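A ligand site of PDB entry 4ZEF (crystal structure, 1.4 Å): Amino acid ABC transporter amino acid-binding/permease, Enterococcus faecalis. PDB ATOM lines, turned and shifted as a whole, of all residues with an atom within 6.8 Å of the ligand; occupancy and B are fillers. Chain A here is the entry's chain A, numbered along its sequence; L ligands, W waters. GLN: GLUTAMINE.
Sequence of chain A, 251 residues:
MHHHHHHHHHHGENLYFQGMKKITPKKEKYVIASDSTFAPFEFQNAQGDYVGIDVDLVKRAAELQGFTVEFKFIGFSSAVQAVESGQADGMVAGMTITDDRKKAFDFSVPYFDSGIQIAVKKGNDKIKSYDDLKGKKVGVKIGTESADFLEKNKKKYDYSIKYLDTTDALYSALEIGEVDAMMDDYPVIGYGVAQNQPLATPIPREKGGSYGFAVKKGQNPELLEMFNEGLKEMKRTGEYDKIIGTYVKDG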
ATOM      1  N   ASP A  35     -35.141 -14.109  14.492  1.00  0.00           N
ATOM      2  CA  ASP A  35     -34.731 -13.986  13.097  1.00  0.00           C
ATOM      3  C   ASP A  35     -34.725 -15.376  12.463  1.00  0.00           C
ATOM      4  O   ASP A  35     -34.784 -16.375  13.150  1.00  0.00           O
ATOM      5  CB  ASP A  35     -33.339 -13.314  13.053  1.00  0.00           C
ATOM      6  CG  ASP A  35     -33.034 -12.588  11.751  1.00  0.00           C
ATOM      7  OD1 ASP A  35     -33.611 -12.885  10.686  1.00  0.00           O
ATOM      8  OD2 ASP A  35     -32.134 -11.719  11.782  1.00  0.00           O
ATOM      9  N   THR A  37     -32.261 -16.654  10.048  1.00  0.00           N
ATOM     10  CA  THR A  37     -30.926 -17.242  10.161  1.00  0.00           C
ATOM     11  C   THR A  37     -30.004 -16.092  10.495  1.00  0.00           C
ATOM     12  O   THR A  37     -30.014 -15.030   9.858  1.00  0.00           O
ATOM     13  CB  THR A  37     -30.441 -18.074   8.897  1.00  0.00           C
ATOM     14  OG1 THR A  37     -31.179 -19.312   8.788  1.00  0.00           O
ATOM     15  CG2 THR A  37     -28.947 -18.435   9.018  1.00  0.00           C
ATOM     16  N   PHE A  38     -29.255 -16.284  11.560  1.00  0.00           N
ATOM     17  CA  PHE A  38     -28.412 -15.214  12.067  1.00  0.00           C
ATOM     18  C   PHE A  38     -27.363 -15.901  12.954  1.00  0.00           C
ATOM     19  O   PHE A  38     -27.374 -15.782  14.177  1.00  0.00           O
ATOM     20  CB  PHE A  38     -29.269 -14.222  12.858  1.00  0.00           C
ATOM     21  CG  PHE A  38     -28.611 -12.884  13.133  1.00  0.00           C
ATOM     22  CD1 PHE A  38     -28.171 -12.089  12.080  1.00  0.00           C
ATOM     23  CD2 PHE A  38     -28.505 -12.379  14.430  1.00  0.00           C
ATOM     24  CE1 PHE A  38     -27.600 -10.848  12.321  1.00  0.00           C
ATOM     25  CE2 PHE A  38     -27.953 -11.139  14.647  1.00  0.00           C
ATOM     26  CZ  PHE A  38     -27.510 -10.367  13.603  1.00  0.00           C
ATOM     27  N   GLU A  42     -28.969 -17.639  16.045  1.00  0.00           N
ATOM     28  CA  GLU A  42     -29.973 -18.646  15.679  1.00  0.00           C
ATOM     29  C   GLU A  42     -29.712 -19.109  14.271  1.00  0.00           C
ATOM     30  O   GLU A  42     -29.623 -18.299  13.339  1.00  0.00           O
ATOM     31  CB  GLU A  42     -31.415 -18.133  15.827  1.00  0.00           C
ATOM     32  CG  GLU A  42     -31.711 -16.747  15.236  1.00  0.00           C
ATOM     33  CD  GLU A  42     -31.425 -15.618  16.199  1.00  0.00           C
ATOM     34  OE1 GLU A  42     -31.347 -15.879  17.415  1.00  0.00           O
ATOM     35  OE2 GLU A  42     -31.354 -14.472  15.755  1.00  0.00           O
ATOM     36  N   GLY A  75     -37.949 -13.791  11.122  1.00  0.00           N
ATOM     37  CA  GLY A  75     -37.243 -12.640  10.596  1.00  0.00           C
ATOM     38  C   GLY A  75     -37.212 -11.511  11.608  1.00  0.00           C
ATOM     39  O   GLY A  75     -38.074 -11.437  12.495  1.00  0.00           O
ATOM     40  N   PHE A  76     -36.242 -10.624  11.478  1.00  0.00           N
ATOM     41  CA  PHE A  76     -36.033  -9.599  12.499  1.00  0.00           C
ATOM     42  C   PHE A  76     -37.194  -8.602  12.612  1.00  0.00           C
ATOM     43  O   PHE A  76     -37.798  -8.442  13.695  1.00  0.00           O
ATOM     44  CB  PHE A  76     -34.707  -8.848  12.273  1.00  0.00           C
ATOM     45  CG  PHE A  76     -34.387  -7.854  13.365  1.00  0.00           C
ATOM     46  CD1 PHE A  76     -34.061  -8.287  14.631  1.00  0.00           C
ATOM     47  CD2 PHE A  76     -34.450  -6.494  13.125  1.00  0.00           C
ATOM     48  CE1 PHE A  76     -33.800  -7.410  15.639  1.00  0.00           C
ATOM     49  CE2 PHE A  76     -34.172  -5.592  14.139  1.00  0.00           C
ATOM     50  CZ  PHE A  76     -33.851  -6.044  15.401  1.00  0.00           C
ATOM     51  N   ALA A  93     -33.117 -12.128  19.074  1.00  0.00           N
ATOM     52  CA  ALA A  93     -32.683 -12.065  17.684  1.00  0.00           C
ATOM     53  C   ALA A  93     -31.426 -11.236  17.551  1.00  0.00           C
ATOM     54  O   ALA A  93     -31.335 -10.363  16.679  1.00  0.00           O
ATOM     55  CB  ALA A  93     -33.812 -11.511  16.790  1.00  0.00           C
ATOM     56  N   GLY A  94     -30.439 -11.502  18.403  1.00  0.00           N
ATOM     57  CA  GLY A  94     -29.259 -10.663  18.466  1.00  0.00           C
ATOM     58  C   GLY A  94     -29.656  -9.195  18.451  1.00  0.00           C
ATOM     59  O   GLY A  94     -29.117  -8.402  17.696  1.00  0.00           O
ATOM     60  N   MET A  95     -30.598  -8.832  19.314  1.00  0.00           N
ATOM     61  CA  MET A  95     -31.222  -7.515  19.251  1.00  0.00           C
ATOM     62  C   MET A  95     -30.529  -6.510  20.158  1.00  0.00           C
ATOM     63  O   MET A  95     -30.487  -6.679  21.381  1.00  0.00           O
ATOM     64  CB  MET A  95     -32.688  -7.640  19.681  1.00  0.00           C
ATOM     65  CG  MET A  95     -33.476  -6.364  19.573  1.00  0.00           C
ATOM     66  SD  MET A  95     -35.158  -6.692  20.132  1.00  0.00           S
ATOM     67  CE  MET A  95     -35.988  -5.220  19.597  1.00  0.00           C
ATOM     68  N   THR A  96     -29.980  -5.460  19.548  1.00  0.00           N
ATOM     69  CA  THR A  96     -29.268  -4.437  20.307  1.00  0.00           C
ATOM     70  C   THR A  96     -30.212  -3.612  21.178  1.00  0.00           C
ATOM     71  O   THR A  96     -31.247  -3.137  20.733  1.00  0.00           O
ATOM     72  CB  THR A  96     -28.525  -3.509  19.341  1.00  0.00           C
ATOM     73  OG1 THR A  96     -27.696  -4.293  18.491  1.00  0.00           O
ATOM     74  CG2 THR A  96     -27.665  -2.484  20.098  1.00  0.00           C
ATOM     75  N   ILE A  97     -29.833  -3.472  22.442  1.00  0.00           N
ATOM     76  CA  ILE A  97     -30.536  -2.588  23.371  1.00  0.00           C
ATOM     77  C   ILE A  97     -30.195  -1.133  23.021  1.00  0.00           C
ATOM     78  O   ILE A  97     -29.026  -0.744  23.024  1.00  0.00           O
ATOM     79  CB  ILE A  97     -30.124  -2.886  24.827  1.00  0.00           C
ATOM     80  CG1 ILE A  97     -30.425  -4.343  25.192  1.00  0.00           C
ATOM     81  CG2 ILE A  97     -30.805  -1.919  25.790  1.00  0.00           C
ATOM     82  CD1 ILE A  97     -29.711  -4.818  26.441  1.00  0.00           C
ATOM     83  N   THR A  98     -31.228  -0.349  22.737  1.00  0.00           N
ATOM     84  CA  THR A  98     -31.057   1.092  22.496  1.00  0.00           C
ATOM     85  C   THR A  98     -32.140   1.897  23.205  1.00  0.00           C
ATOM     86  O   THR A  98     -33.196   1.349  23.530  1.00  0.00           O
ATOM     87  CB  THR A  98     -31.119   1.428  20.987  1.00  0.00           C
ATOM     88  OG1 THR A  98     -32.467   1.289  20.526  1.00  0.00           O
ATOM     89  CG2 THR A  98     -30.202   0.522  20.153  1.00  0.00           C
ATOM     90  N   ARG A 101     -35.465   1.949  21.260  1.00  0.00           N
ATOM     91  CA  ARG A 101     -36.197   0.694  21.373  1.00  0.00           C
ATOM     92  C   ARG A 101     -36.835   0.500  22.751  1.00  0.00           C
ATOM     93  O   ARG A 101     -37.839  -0.211  22.890  1.00  0.00           O
ATOM     94  CB  ARG A 101     -35.297  -0.485  21.020  1.00  0.00           C
ATOM     95  CG  ARG A 101     -35.030  -0.559  19.531  1.00  0.00           C
ATOM     96  CD  ARG A 101     -33.906  -1.533  19.212  1.00  0.00           C
ATOM     97  NE  ARG A 101     -33.779  -1.712  17.773  1.00  0.00           N
ATOM     98  CZ  ARG A 101     -32.913  -2.540  17.186  1.00  0.00           C
ATOM     99  NH1 ARG A 101     -32.069  -3.259  17.911  1.00  0.00           N
ATOM    100  NH2 ARG A 101     -32.890  -2.646  15.865  1.00  0.00           N
ATOM    101  N   SER A 114     -21.656  -6.545  21.258  1.00  0.00           N
ATOM    102  CA  SER A 114     -21.569  -6.649  19.813  1.00  0.00           C
ATOM    103  C   SER A 114     -21.334  -5.287  19.173  1.00  0.00           C
ATOM    104  O   SER A 114     -20.758  -4.380  19.788  1.00  0.00           O
ATOM    105  CB  SER A 114     -22.845  -7.312  19.283  1.00  0.00           C
ATOM    106  OG  SER A 114     -22.692  -7.734  17.938  1.00  0.00           O
ATOM    107  N   GLY A 115     -21.780  -5.149  17.926  1.00  0.00           N
ATOM    108  CA  GLY A 115     -21.432  -4.029  17.097  1.00  0.00           C
ATOM    109  C   GLY A 115     -21.563  -4.450  15.645  1.00  0.00           C
ATOM    110  O   GLY A 115     -21.952  -5.586  15.349  1.00  0.00           O
ATOM    111  N   ILE A 116     -21.245  -3.528  14.736  1.00  0.00           N
ATOM    112  CA  ILE A 116     -21.444  -3.746  13.312  1.00  0.00           C
ATOM    113  C   ILE A 116     -20.126  -3.611  12.560  1.00  0.00           C
ATOM    114  O   ILE A 116     -19.178  -2.976  13.044  1.00  0.00           O
ATOM    115  CB  ILE A 116     -22.522  -2.776  12.741  1.00  0.00           C
ATOM    116  CG1 ILE A 116     -22.079  -1.324  12.871  1.00  0.00           C
ATOM    117  CG2 ILE A 116     -23.859  -2.992  13.440  1.00  0.00           C
ATOM    118  CD1 ILE A 116     -22.998  -0.347  12.180  1.00  0.00           C
ATOM    119  N   LYS A 141     -29.479  -5.297   6.008  1.00  0.00           N
ATOM    120  CA  LYS A 141     -30.773  -5.805   6.431  1.00  0.00           C
ATOM    121  C   LYS A 141     -31.638  -4.640   6.939  1.00  0.00           C
ATOM    122  O   LYS A 141     -31.240  -3.898   7.835  1.00  0.00           O
ATOM    123  CB  LYS A 141     -30.602  -6.859   7.517  1.00  0.00           C
ATOM    124  CG  LYS A 141     -31.900  -7.558   7.955  1.00  0.00           C
ATOM    125  CD  LYS A 141     -31.712  -8.473   9.193  1.00  0.00           C
ATOM    126  CE  LYS A 141     -30.599  -9.492   8.969  1.00  0.00           C
ATOM    127  NZ  LYS A 141     -30.321 -10.410  10.136  1.00  0.00           N
ATOM    128  N   ILE A 142     -32.817  -4.489   6.343  1.00  0.00           N
ATOM    129  CA  ILE A 142     -33.746  -3.434   6.737  1.00  0.00           C
ATOM    130  C   ILE A 142     -34.085  -3.531   8.236  1.00  0.00           C
ATOM    131  O   ILE A 142     -34.151  -4.625   8.809  1.00  0.00           O
ATOM    132  CB  ILE A 142     -35.019  -3.548   5.861  1.00  0.00           C
ATOM    133  CG1 ILE A 142     -35.882  -2.291   5.934  1.00  0.00           C
ATOM    134  CG2 ILE A 142     -35.842  -4.787   6.229  1.00  0.00           C
ATOM    135  CD1 ILE A 142     -36.850  -2.232   4.773  1.00  0.00           C
ATOM    136  N   GLY A 143     -34.216  -2.384   8.895  1.00  0.00           N
ATOM    137  CA  GLY A 143     -34.697  -2.367  10.259  1.00  0.00           C
ATOM    138  C   GLY A 143     -33.632  -2.439  11.338  1.00  0.00           C
ATOM    139  O   GLY A 143     -33.968  -2.403  12.530  1.00  0.00           O
ATOM    140  N   THR A 144     -32.367  -2.484  10.943  1.00  0.00           N
ATOM    141  CA  THR A 144     -31.283  -2.822  11.879  1.00  0.00           C
ATOM    142  C   THR A 144     -30.379  -1.659  12.233  1.00  0.00           C
ATOM    143  O   THR A 144     -30.411  -0.594  11.613  1.00  0.00           O
ATOM    144  CB  THR A 144     -30.375  -3.901  11.286  1.00  0.00           C
ATOM    145  OG1 THR A 144     -29.744  -3.389  10.100  1.00  0.00           O
ATOM    146  CG2 THR A 144     -31.188  -5.170  10.981  1.00  0.00           C
ATOM    147  N   GLU A 145     -29.527  -1.918  13.211  1.00  0.00           N
ATOM    148  CA  GLU A 145     -28.510  -0.963  13.613  1.00  0.00           C
ATOM    149  C   GLU A 145     -27.556  -0.693  12.457  1.00  0.00           C
ATOM    150  O   GLU A 145     -27.092   0.448  12.275  1.00  0.00           O
ATOM    151  CB  GLU A 145     -27.753  -1.509  14.837  1.00  0.00           C
ATOM    152  CG  GLU A 145     -28.656  -1.609  16.092  1.00  0.00           C
ATOM    153  CD  GLU A 145     -29.311  -0.261  16.477  1.00  0.00           C
ATOM    154  OE1 GLU A 145     -28.554   0.615  16.837  1.00  0.00           O
ATOM    155  OE2 GLU A 145     -30.570  -0.074  16.435  1.00  0.00           O
ATOM    156  N   SER A 146     -27.259  -1.714  11.642  1.00  0.00           N
ATOM    157  CA  SER A 146     -26.430  -1.488  10.455  1.00  0.00           C
ATOM    158  C   SER A 146     -27.081  -0.507   9.472  1.00  0.00           C
ATOM    159  O   SER A 146     -26.423   0.398   8.919  1.00  0.00           O
ATOM    160  CB  SER A 146     -26.122  -2.801   9.736  1.00  0.00           C
ATOM    161  OG  SER A 146     -25.197  -3.606  10.460  1.00  0.00           O
ATOM    162  N   ASP A 148     -29.174   1.876  10.144  1.00  0.00           N
ATOM    163  CA  ASP A 148     -29.128   3.216  10.738  1.00  0.00           C
ATOM    164  C   ASP A 148     -27.764   3.850  10.523  1.00  0.00           C
ATOM    165  O   ASP A 148     -27.662   5.037  10.220  1.00  0.00           O
ATOM    166  CB  ASP A 148     -29.442   3.165  12.236  1.00  0.00           C
ATOM    167  CG  ASP A 148     -30.899   2.809  12.515  1.00  0.00           C
ATOM    168  OD1 ASP A 148     -31.742   2.826  11.589  1.00  0.00           O
ATOM    169  OD2 ASP A 148     -31.195   2.509  13.699  1.00  0.00           O
ATOM    170  N   THR A 167     -29.818 -12.111   6.629  1.00  0.00           N
ATOM    171  CA  THR A 167     -28.364 -12.126   6.566  1.00  0.00           C
ATOM    172  C   THR A 167     -27.905 -13.047   5.439  1.00  0.00           C
ATOM    173  O   THR A 167     -26.909 -12.740   4.760  1.00  0.00           O
ATOM    174  CB  THR A 167     -27.788 -12.531   7.947  1.00  0.00           C
ATOM    175  OG1 THR A 167     -28.019 -11.463   8.878  1.00  0.00           O
ATOM    176  CG2 THR A 167     -26.310 -12.824   7.872  1.00  0.00           C
ATOM    177  N   ASP A 184     -23.257  -5.829   8.612  1.00  0.00           N
ATOM    178  CA  ASP A 184     -24.015  -6.681   9.525  1.00  0.00           C
ATOM    179  C   ASP A 184     -23.273  -6.745  10.849  1.00  0.00           C
ATOM    180  O   ASP A 184     -22.227  -6.118  11.020  1.00  0.00           O
ATOM    181  CB  ASP A 184     -24.246  -8.058   8.893  1.00  0.00           C
ATOM    182  CG  ASP A 184     -25.492  -8.765   9.418  1.00  0.00           C
ATOM    183  OD1 ASP A 184     -25.991  -8.459  10.522  1.00  0.00           O
ATOM    184  OD2 ASP A 184     -26.002  -9.660   8.691  1.00  0.00           O
ATOM    185  N   ASP A 185     -23.819  -7.466  11.816  1.00  0.00           N
ATOM    186  CA  ASP A 185     -23.185  -7.509  13.130  1.00  0.00           C
ATOM    187  C   ASP A 185     -21.833  -8.239  13.054  1.00  0.00           C
ATOM    188  O   ASP A 185     -21.701  -9.246  12.373  1.00  0.00           O
ATOM    189  CB  ASP A 185     -24.101  -8.156  14.151  1.00  0.00           C
ATOM    190  CG  ASP A 185     -25.233  -7.242  14.593  1.00  0.00           C
ATOM    191  OD1 ASP A 185     -25.403  -6.128  14.044  1.00  0.00           O
ATOM    192  OD2 ASP A 185     -25.957  -7.653  15.516  1.00  0.00           O
ATOM    193  N   TYR A 211     -26.629  -7.037  23.272  1.00  0.00           N
ATOM    194  CA  TYR A 211     -27.886  -7.678  22.962  1.00  0.00           C
ATOM    195  C   TYR A 211     -28.737  -7.926  24.195  1.00  0.00           C
ATOM    196  O   TYR A 211     -28.218  -8.184  25.283  1.00  0.00           O
ATOM    197  CB  TYR A 211     -27.650  -9.035  22.310  1.00  0.00           C
ATOM    198  CG  TYR A 211     -26.941  -9.047  20.985  1.00  0.00           C
ATOM    199  CD1 TYR A 211     -26.820  -7.903  20.202  1.00  0.00           C
ATOM    200  CD2 TYR A 211     -26.374 -10.221  20.520  1.00  0.00           C
ATOM    201  CE1 TYR A 211     -26.168  -7.944  18.958  1.00  0.00           C
ATOM    202  CE2 TYR A 211     -25.731 -10.286  19.302  1.00  0.00           C
ATOM    203  CZ  TYR A 211     -25.611  -9.141  18.519  1.00  0.00           C
ATOM    204  OH  TYR A 211     -24.937  -9.238  17.321  1.00  0.00           O
HETATM  205  N   GLN L   1     -28.093  -6.204  16.317  1.00  0.00           N
HETATM  206  CA  GLN L   1     -28.767  -5.606  15.151  1.00  0.00           C
HETATM  207  C   GLN L   1     -30.008  -4.884  15.606  1.00  0.00           C
HETATM  208  O   GLN L   1     -30.478  -5.109  16.757  1.00  0.00           O
HETATM  209  CB  GLN L   1     -29.102  -6.678  14.108  1.00  0.00           C
HETATM  210  CG  GLN L   1     -30.143  -7.717  14.525  1.00  0.00           C
HETATM  211  CD  GLN L   1     -30.447  -8.703  13.416  1.00  0.00           C
HETATM  212  OE1 GLN L   1     -30.149  -8.467  12.234  1.00  0.00           O
HETATM  213  NE2 GLN L   1     -31.051  -9.835  13.785  1.00  0.00           N
HETATM  214  OXT GLN L   1     -30.550  -4.080  14.817  1.00  0.00           O
HETATM  215  O   HOH W   1     -26.961  -4.841  12.143  1.00  0.00           O
HETATM  216  O   HOH W   2     -25.568  -4.262  16.283  1.00  0.00           O
HETATM  217  O   HOH W   3     -28.189  -7.015  10.817  1.00  0.00           O
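The backbone NH (N) of Thr 96 is in hydrogen-bond range of an oxygen (O) of the ligand, at 2.9 Å.
The side-chain carboxylate of Asp 35 sits at hydrogen-bond distance from a nitrogen (NE2) of the ligand, 3.0 Å away.
The guanidinium group (NH1) of Arg 101 is in salt-bridge range of an oxygen (O) of the ligand.
OD2 of Asp 185 lies within salt-bridge range of N of the ligand.
The backbone carbonyl oxygen (O) of Ala 93 lies within hydrogen-bond range of a nitrogen (NE2) of the ligand, 3.0 Å away.
A nitrogen (N) of the ligand is in hydrogen-bond range of the side-chain hydroxyl of Thr 96 (2.9 Å).
NZ of Lys 141 is in hydrogen-bond range of OE1 of the ligand, at 2.9 Å.
N of the ligand is in hydrogen-bond range of O of Gly 94 (2.8 Å).
The backbone NH (N) of Glu 145 lies within hydrogen-bond range of an oxygen (OXT) of the ligand.
OD2 of Asp 185 lies within hydrogen-bond range of OH of Tyr 211 (2.6 Å).
OH of Tyr 211 lies within hydrogen-bond range of OG of Ser 114, at 2.8 Å.
The side-chain hydroxyl of Thr 144 lies within hydrogen-bond range of the backbone carbonyl oxygen of Lys 141 (2.8 Å).
The side-chain amino group (NZ) of Lys 141 is in salt-bridge range of the side-chain carboxylate (OD2) of Asp 35 (2.8 Å).
The side-chain amino group (NZ) of Lys 141 sits at hydrogen-bond distance from the side-chain hydroxyl (OG1) of Thr 167, 2.8 Å away.
The side-chain hydroxyl (OG1) of Thr 144 sits close to the backbone NH (N) of Ser 146 (3.4 Å).
The backbone NH of Arg 101 sits at hydrogen-bond distance from the side-chain hydroxyl of Thr 98, at 3.2 Å.
NH1 of Arg 101 sits at hydrogen-bond distance from O of Thr 96, at 2.9 Å.
CZ of Phe 38 touches CD of the ligand, at 3.4 Å.
Phe 76 touches the ligand.
Met 95 touches the ligand (CA to O, 3.5 Å).
Thr 144 touches the ligand.
Tyr 211 touches the ligand (CE1 to N, 3.7 Å).
Hydrophobic or aromatic side chains within 4 Å of the ligand: Phe 38, Phe 76 and Tyr 211.
Within 4 Å of the ligand: Asp 35, Phe 38, Phe 76, Ala 93, Gly 94, Met 95, Thr 96, Arg 101, Lys 141, Thr 144, Glu 145, Asp 185 and Tyr 211.
Water W3 bridges OD1 of Asp 184 and OE1 of the ligand.
Water W2 lies within hydrogen-bond range of the side-chain carboxylate (OD1) of Asp 185 (2.9 Å), the side-chain hydroxyl (OG1) of Thr 96 (3.1 Å) and a nitrogen (N) of the ligand (3.2 Å).
Water W1 lies within hydrogen-bond range of OG of Ser 146 (2.7 Å) and OD1 of Asp 185 (2.8 Å).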
